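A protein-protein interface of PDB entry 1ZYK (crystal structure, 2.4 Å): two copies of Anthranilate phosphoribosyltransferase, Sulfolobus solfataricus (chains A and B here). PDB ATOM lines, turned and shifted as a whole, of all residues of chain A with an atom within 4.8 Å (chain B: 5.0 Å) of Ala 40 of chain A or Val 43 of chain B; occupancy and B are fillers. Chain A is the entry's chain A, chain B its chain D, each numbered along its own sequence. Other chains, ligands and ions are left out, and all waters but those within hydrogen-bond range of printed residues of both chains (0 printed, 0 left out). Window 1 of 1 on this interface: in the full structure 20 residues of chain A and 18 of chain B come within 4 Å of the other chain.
OG of Ser 39 of chain B sits at hydrogen-bond distance from O of Ile 36 of chain A (2.8 Å).
CD2 of Leu 7 of chain A touches O of Leu 167 of chain B, at 3.8 Å.
CD1 of Ile 11 of chain A touches CG1 of Val 43 of chain B, 3.6 Å away.
NE of Arg 46 of chain B touches CG2 of Ile 11 of chain A (3.2 Å).
CD1 of Ile 11 of chain A touches SD of Met 47 of chain B, at 3.9 Å.
Leu 37 of chain A touches Leu 167 of chain B.
Ser 39 of chain B touches Ala 40 of chain A.
Ala 40 of chain A touches Val 43 of chain B (CB to CG2, 3.6 Å).
Leu 167 of chain B touches Ala 40 of chain A (CD2 to CB, 3.5 Å).
Val 43 of chain A touches Ala 40 of chain B.
Met 47 of chain B touches Ala 44 of chain A.
Of chain B, only Ser 39, Val 43 and Leu 167 come within 4 Å of Ala 40 of chain A.
Val 43 of chain B touches just these residues of chain A: Ile 11 (3.6 Å) and Ala 40 (3.6 Å).
Printed residues of chain B within 4 Å of Ile 36 of chain A: Ser 39 (2.8 Å).
Printed residues of chain A within 4 Å of Ile 169 of chain B: Leu 7.
Of the printed residues of chain A, Ala 40 of chain B touches Ser 39 (3.7 Å) and Val 43 (3.5 Å).
Of the printed residues of chain B, Val 43 of chain A touches Ala 40 (3.5 Å).
Lys 48 of chain B touches none of the printed residues of chain A.
Val 38 of chain A touches none of the printed residues of chain B.
The nearest printed residue of chain B that does not touch Ala 40 of chain A is Ala 40 of chain B (5.3 Å).
Of the 12 printed residues of chain A, 8 touch a printed residue of chain B.
Printed residues of chain A that touch a printed residue of chain B: Leu 7, Ile 11, Ile 36, Leu 37, Ser 39, Ala 40, Val 43 and Ala 44.
Hydrophobic or aromatic side chains of chain A within 4 Å of the printed part of chain B: Leu 7, Ile 11, Ile 36, Leu 37, Ala 40, Val 43 and Ala 44.
Of the 12 printed residues of chain B, 7 touch a printed residue of chain A.
Hydrophobic or aromatic side chains of chain B within 4 Å of the printed part of chain A: Ala 40, Val 43, Met 47, Leu 167 and Ile 169.
Ser 39 of chain A touches Ala 40 of chain B, and with the chains exchanged Ala 40 of chain A touches Ser 39 of chain B.
Ala 40 of chain A touches Val 43 of chain B, and with the chains exchanged Val 43 of chain A touches Ala 40 of chain B.
Of the 13 pairs that touch across the chains among the printed residues, 4 have their exchanged pair printed and touching as well.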
ATOM      1  N   LEU A   7     -16.163   7.138  26.315  1.00  0.00           N
ATOM      2  CA  LEU A   7     -17.582   7.452  26.354  1.00  0.00           C
ATOM      3  C   LEU A   7     -18.399   6.299  26.938  1.00  0.00           C
ATOM      4  O   LEU A   7     -19.174   6.494  27.882  1.00  0.00           O
ATOM      5  CB  LEU A   7     -18.080   7.792  24.950  1.00  0.00           C
ATOM      6  CG  LEU A   7     -19.566   8.128  24.870  1.00  0.00           C
ATOM      7  CD1 LEU A   7     -19.896   9.247  25.854  1.00  0.00           C
ATOM      8  CD2 LEU A   7     -19.921   8.534  23.447  1.00  0.00           C
ATOM      9  N   ILE A  11     -20.746   6.299  30.118  1.00  0.00           N
ATOM     10  CA  ILE A  11     -22.164   5.964  30.000  1.00  0.00           C
ATOM     11  C   ILE A  11     -22.497   4.888  31.028  1.00  0.00           C
ATOM     12  O   ILE A  11     -23.611   4.840  31.531  1.00  0.00           O
ATOM     13  CB  ILE A  11     -22.527   5.420  28.595  1.00  0.00           C
ATOM     14  CG1 ILE A  11     -22.235   6.470  27.520  1.00  0.00           C
ATOM     15  CG2 ILE A  11     -23.998   5.048  28.557  1.00  0.00           C
ATOM     16  CD1 ILE A  11     -23.091   7.703  27.619  1.00  0.00           C
ATOM     17  N   ILE A  36     -19.899  16.601  18.413  1.00  0.00           N
ATOM     18  CA  ILE A  36     -20.910  15.633  18.822  1.00  0.00           C
ATOM     19  C   ILE A  36     -20.415  14.779  19.991  1.00  0.00           C
ATOM     20  O   ILE A  36     -21.174  14.485  20.915  1.00  0.00           O
ATOM     21  CB  ILE A  36     -21.297  14.713  17.640  1.00  0.00           C
ATOM     22  CG1 ILE A  36     -22.230  15.465  16.691  1.00  0.00           C
ATOM     23  CG2 ILE A  36     -21.943  13.450  18.155  1.00  0.00           C
ATOM     24  CD1 ILE A  36     -22.348  14.848  15.317  1.00  0.00           C
ATOM     25  N   LEU A  37     -19.141  14.394  19.951  1.00  0.00           N
ATOM     26  CA  LEU A  37     -18.553  13.577  21.006  1.00  0.00           C
ATOM     27  C   LEU A  37     -18.191  14.410  22.229  1.00  0.00           C
ATOM     28  O   LEU A  37     -18.318  13.947  23.369  1.00  0.00           O
ATOM     29  CB  LEU A  37     -17.304  12.854  20.500  1.00  0.00           C
ATOM     30  CG  LEU A  37     -17.544  11.672  19.562  1.00  0.00           C
ATOM     31  CD1 LEU A  37     -16.216  11.168  19.002  1.00  0.00           C
ATOM     32  CD2 LEU A  37     -18.265  10.573  20.312  1.00  0.00           C
ATOM     33  N   VAL A  38     -17.728  15.633  22.004  1.00  0.00           N
ATOM     34  CA  VAL A  38     -17.385  16.489  23.134  1.00  0.00           C
ATOM     35  C   VAL A  38     -18.659  16.726  23.932  1.00  0.00           C
ATOM     36  O   VAL A  38     -18.655  16.680  25.158  1.00  0.00           O
ATOM     37  CB  VAL A  38     -16.812  17.843  22.675  1.00  0.00           C
ATOM     38  CG1 VAL A  38     -16.746  18.818  23.852  1.00  0.00           C
ATOM     39  CG2 VAL A  38     -15.426  17.629  22.089  1.00  0.00           C
ATOM     40  N   SER A  39     -19.751  16.959  23.216  1.00  0.00           N
ATOM     41  CA  SER A  39     -21.045  17.183  23.829  1.00  0.00           C
ATOM     42  C   SER A  39     -21.492  15.962  24.635  1.00  0.00           C
ATOM     43  O   SER A  39     -21.969  16.094  25.763  1.00  0.00           O
ATOM     44  CB  SER A  39     -22.082  17.496  22.753  1.00  0.00           C
ATOM     45  OG  SER A  39     -23.366  17.636  23.328  1.00  0.00           O
ATOM     46  N   ALA A  40     -21.351  14.769  24.060  1.00  0.00           N
ATOM     47  CA  ALA A  40     -21.742  13.545  24.770  1.00  0.00           C
ATOM     48  C   ALA A  40     -20.882  13.355  26.018  1.00  0.00           C
ATOM     49  O   ALA A  40     -21.391  13.024  27.094  1.00  0.00           O
ATOM     50  CB  ALA A  40     -21.600  12.322  23.866  1.00  0.00           C
ATOM     51  N   ILE A  41     -19.575  13.553  25.868  1.00  0.00           N
ATOM     52  CA  ILE A  41     -18.646  13.408  26.987  1.00  0.00           C
ATOM     53  C   ILE A  41     -19.027  14.301  28.163  1.00  0.00           C
ATOM     54  O   ILE A  41     -19.142  13.838  29.292  1.00  0.00           O
ATOM     55  CB  ILE A  41     -17.189  13.768  26.575  1.00  0.00           C
ATOM     56  CG1 ILE A  41     -16.598  12.675  25.682  1.00  0.00           C
ATOM     57  CG2 ILE A  41     -16.332  13.956  27.809  1.00  0.00           C
ATOM     58  CD1 ILE A  41     -16.476  11.310  26.369  1.00  0.00           C
ATOM     59  N   LEU A  42     -19.226  15.587  27.895  1.00  0.00           N
ATOM     60  CA  LEU A  42     -19.565  16.519  28.965  1.00  0.00           C
ATOM     61  C   LEU A  42     -20.891  16.177  29.642  1.00  0.00           C
ATOM     62  O   LEU A  42     -21.002  16.252  30.871  1.00  0.00           O
ATOM     63  CB  LEU A  42     -19.571  17.957  28.432  1.00  0.00           C
ATOM     64  CG  LEU A  42     -18.229  18.409  27.821  1.00  0.00           C
ATOM     65  CD1 LEU A  42     -18.308  19.865  27.452  1.00  0.00           C
ATOM     66  CD2 LEU A  42     -17.087  18.184  28.809  1.00  0.00           C
ATOM     67  N   VAL A  43     -21.885  15.775  28.855  1.00  0.00           N
ATOM     68  CA  VAL A  43     -23.178  15.405  29.421  1.00  0.00           C
ATOM     69  C   VAL A  43     -23.084  14.137  30.276  1.00  0.00           C
ATOM     70  O   VAL A  43     -23.645  14.081  31.366  1.00  0.00           O
ATOM     71  CB  VAL A  43     -24.223  15.199  28.322  1.00  0.00           C
ATOM     72  CG1 VAL A  43     -25.490  14.606  28.914  1.00  0.00           C
ATOM     73  CG2 VAL A  43     -24.523  16.532  27.650  1.00  0.00           C
ATOM     74  N   ALA A  44     -22.362  13.129  29.798  1.00  0.00           N
ATOM     75  CA  ALA A  44     -22.232  11.881  30.557  1.00  0.00           C
ATOM     76  C   ALA A  44     -21.516  12.175  31.862  1.00  0.00           C
ATOM     77  O   ALA A  44     -21.914  11.713  32.933  1.00  0.00           O
ATOM     78  CB  ALA A  44     -21.439  10.845  29.757  1.00  0.00           C
ATOM     79  N   LEU A  45     -20.459  12.967  31.758  1.00  0.00           N
ATOM     80  CA  LEU A  45     -19.657  13.343  32.912  1.00  0.00           C
ATOM     81  C   LEU A  45     -20.538  13.999  33.962  1.00  0.00           C
ATOM     82  O   LEU A  45     -20.407  13.708  35.147  1.00  0.00           O
ATOM     83  CB  LEU A  45     -18.542  14.308  32.487  1.00  0.00           C
ATOM     84  CG  LEU A  45     -17.074  14.023  32.815  1.00  0.00           C
ATOM     85  CD1 LEU A  45     -16.813  12.550  32.992  1.00  0.00           C
ATOM     86  CD2 LEU A  45     -16.222  14.571  31.690  1.00  0.00           C
ATOM     87  N   SER B  39     -27.186  15.104  20.316  1.00  0.00           N
ATOM     88  CA  SER B  39     -26.224  14.225  20.966  1.00  0.00           C
ATOM     89  C   SER B  39     -26.418  14.222  22.469  1.00  0.00           C
ATOM     90  O   SER B  39     -26.473  13.160  23.096  1.00  0.00           O
ATOM     91  CB  SER B  39     -24.791  14.662  20.639  1.00  0.00           C
ATOM     92  OG  SER B  39     -23.857  13.759  21.208  1.00  0.00           O
ATOM     93  N   ALA B  40     -26.515  15.411  23.050  1.00  0.00           N
ATOM     94  CA  ALA B  40     -26.695  15.530  24.495  1.00  0.00           C
ATOM     95  C   ALA B  40     -27.990  14.861  24.938  1.00  0.00           C
ATOM     96  O   ALA B  40     -28.022  14.167  25.954  1.00  0.00           O
ATOM     97  CB  ALA B  40     -26.696  16.986  24.901  1.00  0.00           C
ATOM     98  N   ILE B  41     -29.062  15.066  24.181  1.00  0.00           N
ATOM     99  CA  ILE B  41     -30.334  14.452  24.550  1.00  0.00           C
ATOM    100  C   ILE B  41     -30.309  12.923  24.475  1.00  0.00           C
ATOM    101  O   ILE B  41     -30.860  12.260  25.352  1.00  0.00           O
ATOM    102  CB  ILE B  41     -31.491  15.009  23.700  1.00  0.00           C
ATOM    103  CG1 ILE B  41     -31.815  16.431  24.174  1.00  0.00           C
ATOM    104  CG2 ILE B  41     -32.718  14.102  23.811  1.00  0.00           C
ATOM    105  CD1 ILE B  41     -32.977  17.072  23.459  1.00  0.00           C
ATOM    106  N   LEU B  42     -29.665  12.359  23.453  1.00  0.00           N
ATOM    107  CA  LEU B  42     -29.580  10.896  23.335  1.00  0.00           C
ATOM    108  C   LEU B  42     -28.766  10.301  24.505  1.00  0.00           C
ATOM    109  O   LEU B  42     -29.100   9.239  25.042  1.00  0.00           O
ATOM    110  CB  LEU B  42     -28.947  10.493  21.992  1.00  0.00           C
ATOM    111  CG  LEU B  42     -29.743  10.802  20.707  1.00  0.00           C
ATOM    112  CD1 LEU B  42     -28.962  10.354  19.490  1.00  0.00           C
ATOM    113  CD2 LEU B  42     -31.091  10.105  20.735  1.00  0.00           C
ATOM    114  N   VAL B  43     -27.708  10.993  24.914  1.00  0.00           N
ATOM    115  CA  VAL B  43     -26.891  10.504  26.014  1.00  0.00           C
ATOM    116  C   VAL B  43     -27.628  10.644  27.344  1.00  0.00           C
ATOM    117  O   VAL B  43     -27.647   9.711  28.154  1.00  0.00           O
ATOM    118  CB  VAL B  43     -25.550  11.243  26.072  1.00  0.00           C
ATOM    119  CG1 VAL B  43     -24.820  10.898  27.345  1.00  0.00           C
ATOM    120  CG2 VAL B  43     -24.700  10.853  24.857  1.00  0.00           C
ATOM    121  N   ALA B  44     -28.253  11.802  27.558  1.00  0.00           N
ATOM    122  CA  ALA B  44     -29.003  12.054  28.779  1.00  0.00           C
ATOM    123  C   ALA B  44     -30.151  11.056  28.882  1.00  0.00           C
ATOM    124  O   ALA B  44     -30.438  10.517  29.951  1.00  0.00           O
ATOM    125  CB  ALA B  44     -29.551  13.463  28.762  1.00  0.00           C
ATOM    126  N   LEU B  45     -30.809  10.818  27.753  1.00  0.00           N
ATOM    127  CA  LEU B  45     -31.934   9.890  27.695  1.00  0.00           C
ATOM    128  C   LEU B  45     -31.467   8.498  28.125  1.00  0.00           C
ATOM    129  O   LEU B  45     -32.133   7.825  28.912  1.00  0.00           O
ATOM    130  CB  LEU B  45     -32.493   9.867  26.269  1.00  0.00           C
ATOM    131  CG  LEU B  45     -33.988   9.696  25.986  1.00  0.00           C
ATOM    132  CD1 LEU B  45     -34.860  10.194  27.133  1.00  0.00           C
ATOM    133  CD2 LEU B  45     -34.301  10.478  24.714  1.00  0.00           C
ATOM    134  N   ARG B  46     -30.305   8.078  27.631  1.00  0.00           N
ATOM    135  CA  ARG B  46     -29.771   6.767  27.979  1.00  0.00           C
ATOM    136  C   ARG B  46     -29.251   6.668  29.406  1.00  0.00           C
ATOM    137  O   ARG B  46     -29.428   5.642  30.067  1.00  0.00           O
ATOM    138  CB  ARG B  46     -28.644   6.361  27.033  1.00  0.00           C
ATOM    139  CG  ARG B  46     -28.021   5.063  27.474  1.00  0.00           C
ATOM    140  CD  ARG B  46     -26.906   4.603  26.582  1.00  0.00           C
ATOM    141  NE  ARG B  46     -26.331   3.368  27.103  1.00  0.00           N
ATOM    142  CZ  ARG B  46     -25.518   2.573  26.417  1.00  0.00           C
ATOM    143  NH1 ARG B  46     -25.185   2.880  25.170  1.00  0.00           N
ATOM    144  NH2 ARG B  46     -25.024   1.478  26.983  1.00  0.00           N
ATOM    145  N   MET B  47     -28.591   7.715  29.888  1.00  0.00           N
ATOM    146  CA  MET B  47     -28.069   7.666  31.245  1.00  0.00           C
ATOM    147  C   MET B  47     -29.152   7.809  32.294  1.00  0.00           C
ATOM    148  O   MET B  47     -28.980   7.389  33.439  1.00  0.00           O
ATOM    149  CB  MET B  47     -26.973   8.702  31.423  1.00  0.00           C
ATOM    150  CG  MET B  47     -25.809   8.372  30.525  1.00  0.00           C
ATOM    151  SD  MET B  47     -24.339   9.211  30.971  1.00  0.00           S
ATOM    152  CE  MET B  47     -24.156   8.653  32.669  1.00  0.00           C
ATOM    153  N   LYS B  48     -30.276   8.399  31.897  1.00  0.00           N
ATOM    154  CA  LYS B  48     -31.405   8.531  32.802  1.00  0.00           C
ATOM    155  C   LYS B  48     -32.123   7.177  32.778  1.00  0.00           C
ATOM    156  O   LYS B  48     -32.677   6.735  33.786  1.00  0.00           O
ATOM    157  CB  LYS B  48     -32.368   9.612  32.311  1.00  0.00           C
ATOM    158  CG  LYS B  48     -33.669   9.697  33.116  1.00  0.00           C
ATOM    159  CD  LYS B  48     -34.597  10.740  32.531  1.00  0.00           C
ATOM    160  CE  LYS B  48     -35.183  10.284  31.189  1.00  0.00           C
ATOM    161  NZ  LYS B  48     -36.223   9.228  31.383  1.00  0.00           N
ATOM    162  N   LEU B 167     -21.336   9.133  17.532  1.00  0.00           N
ATOM    163  CA  LEU B 167     -21.380   8.708  18.929  1.00  0.00           C
ATOM    164  C   LEU B 167     -20.783   7.315  19.087  1.00  0.00           C
ATOM    165  O   LEU B 167     -19.975   7.068  19.983  1.00  0.00           O
ATOM    166  CB  LEU B 167     -22.820   8.711  19.450  1.00  0.00           C
ATOM    167  CG  LEU B 167     -23.411  10.070  19.841  1.00  0.00           C
ATOM    168  CD1 LEU B 167     -24.870   9.921  20.230  1.00  0.00           C
ATOM    169  CD2 LEU B 167     -22.619  10.637  21.011  1.00  0.00           C
ATOM    170  N   ILE B 169     -22.276   4.606  20.032  1.00  0.00           N
ATOM    171  CA  ILE B 169     -22.780   3.899  21.204  1.00  0.00           C
ATOM    172  C   ILE B 169     -24.253   3.641  20.993  1.00  0.00           C
ATOM    173  O   ILE B 169     -24.866   4.227  20.104  1.00  0.00           O
ATOM    174  CB  ILE B 169     -22.643   4.709  22.525  1.00  0.00           C
ATOM    175  CG1 ILE B 169     -23.477   5.991  22.434  1.00  0.00           C
ATOM    176  CG2 ILE B 169     -21.180   4.991  22.825  1.00  0.00           C
ATOM    177  CD1 ILE B 169     -23.711   6.677  23.765  1.00  0.00           C
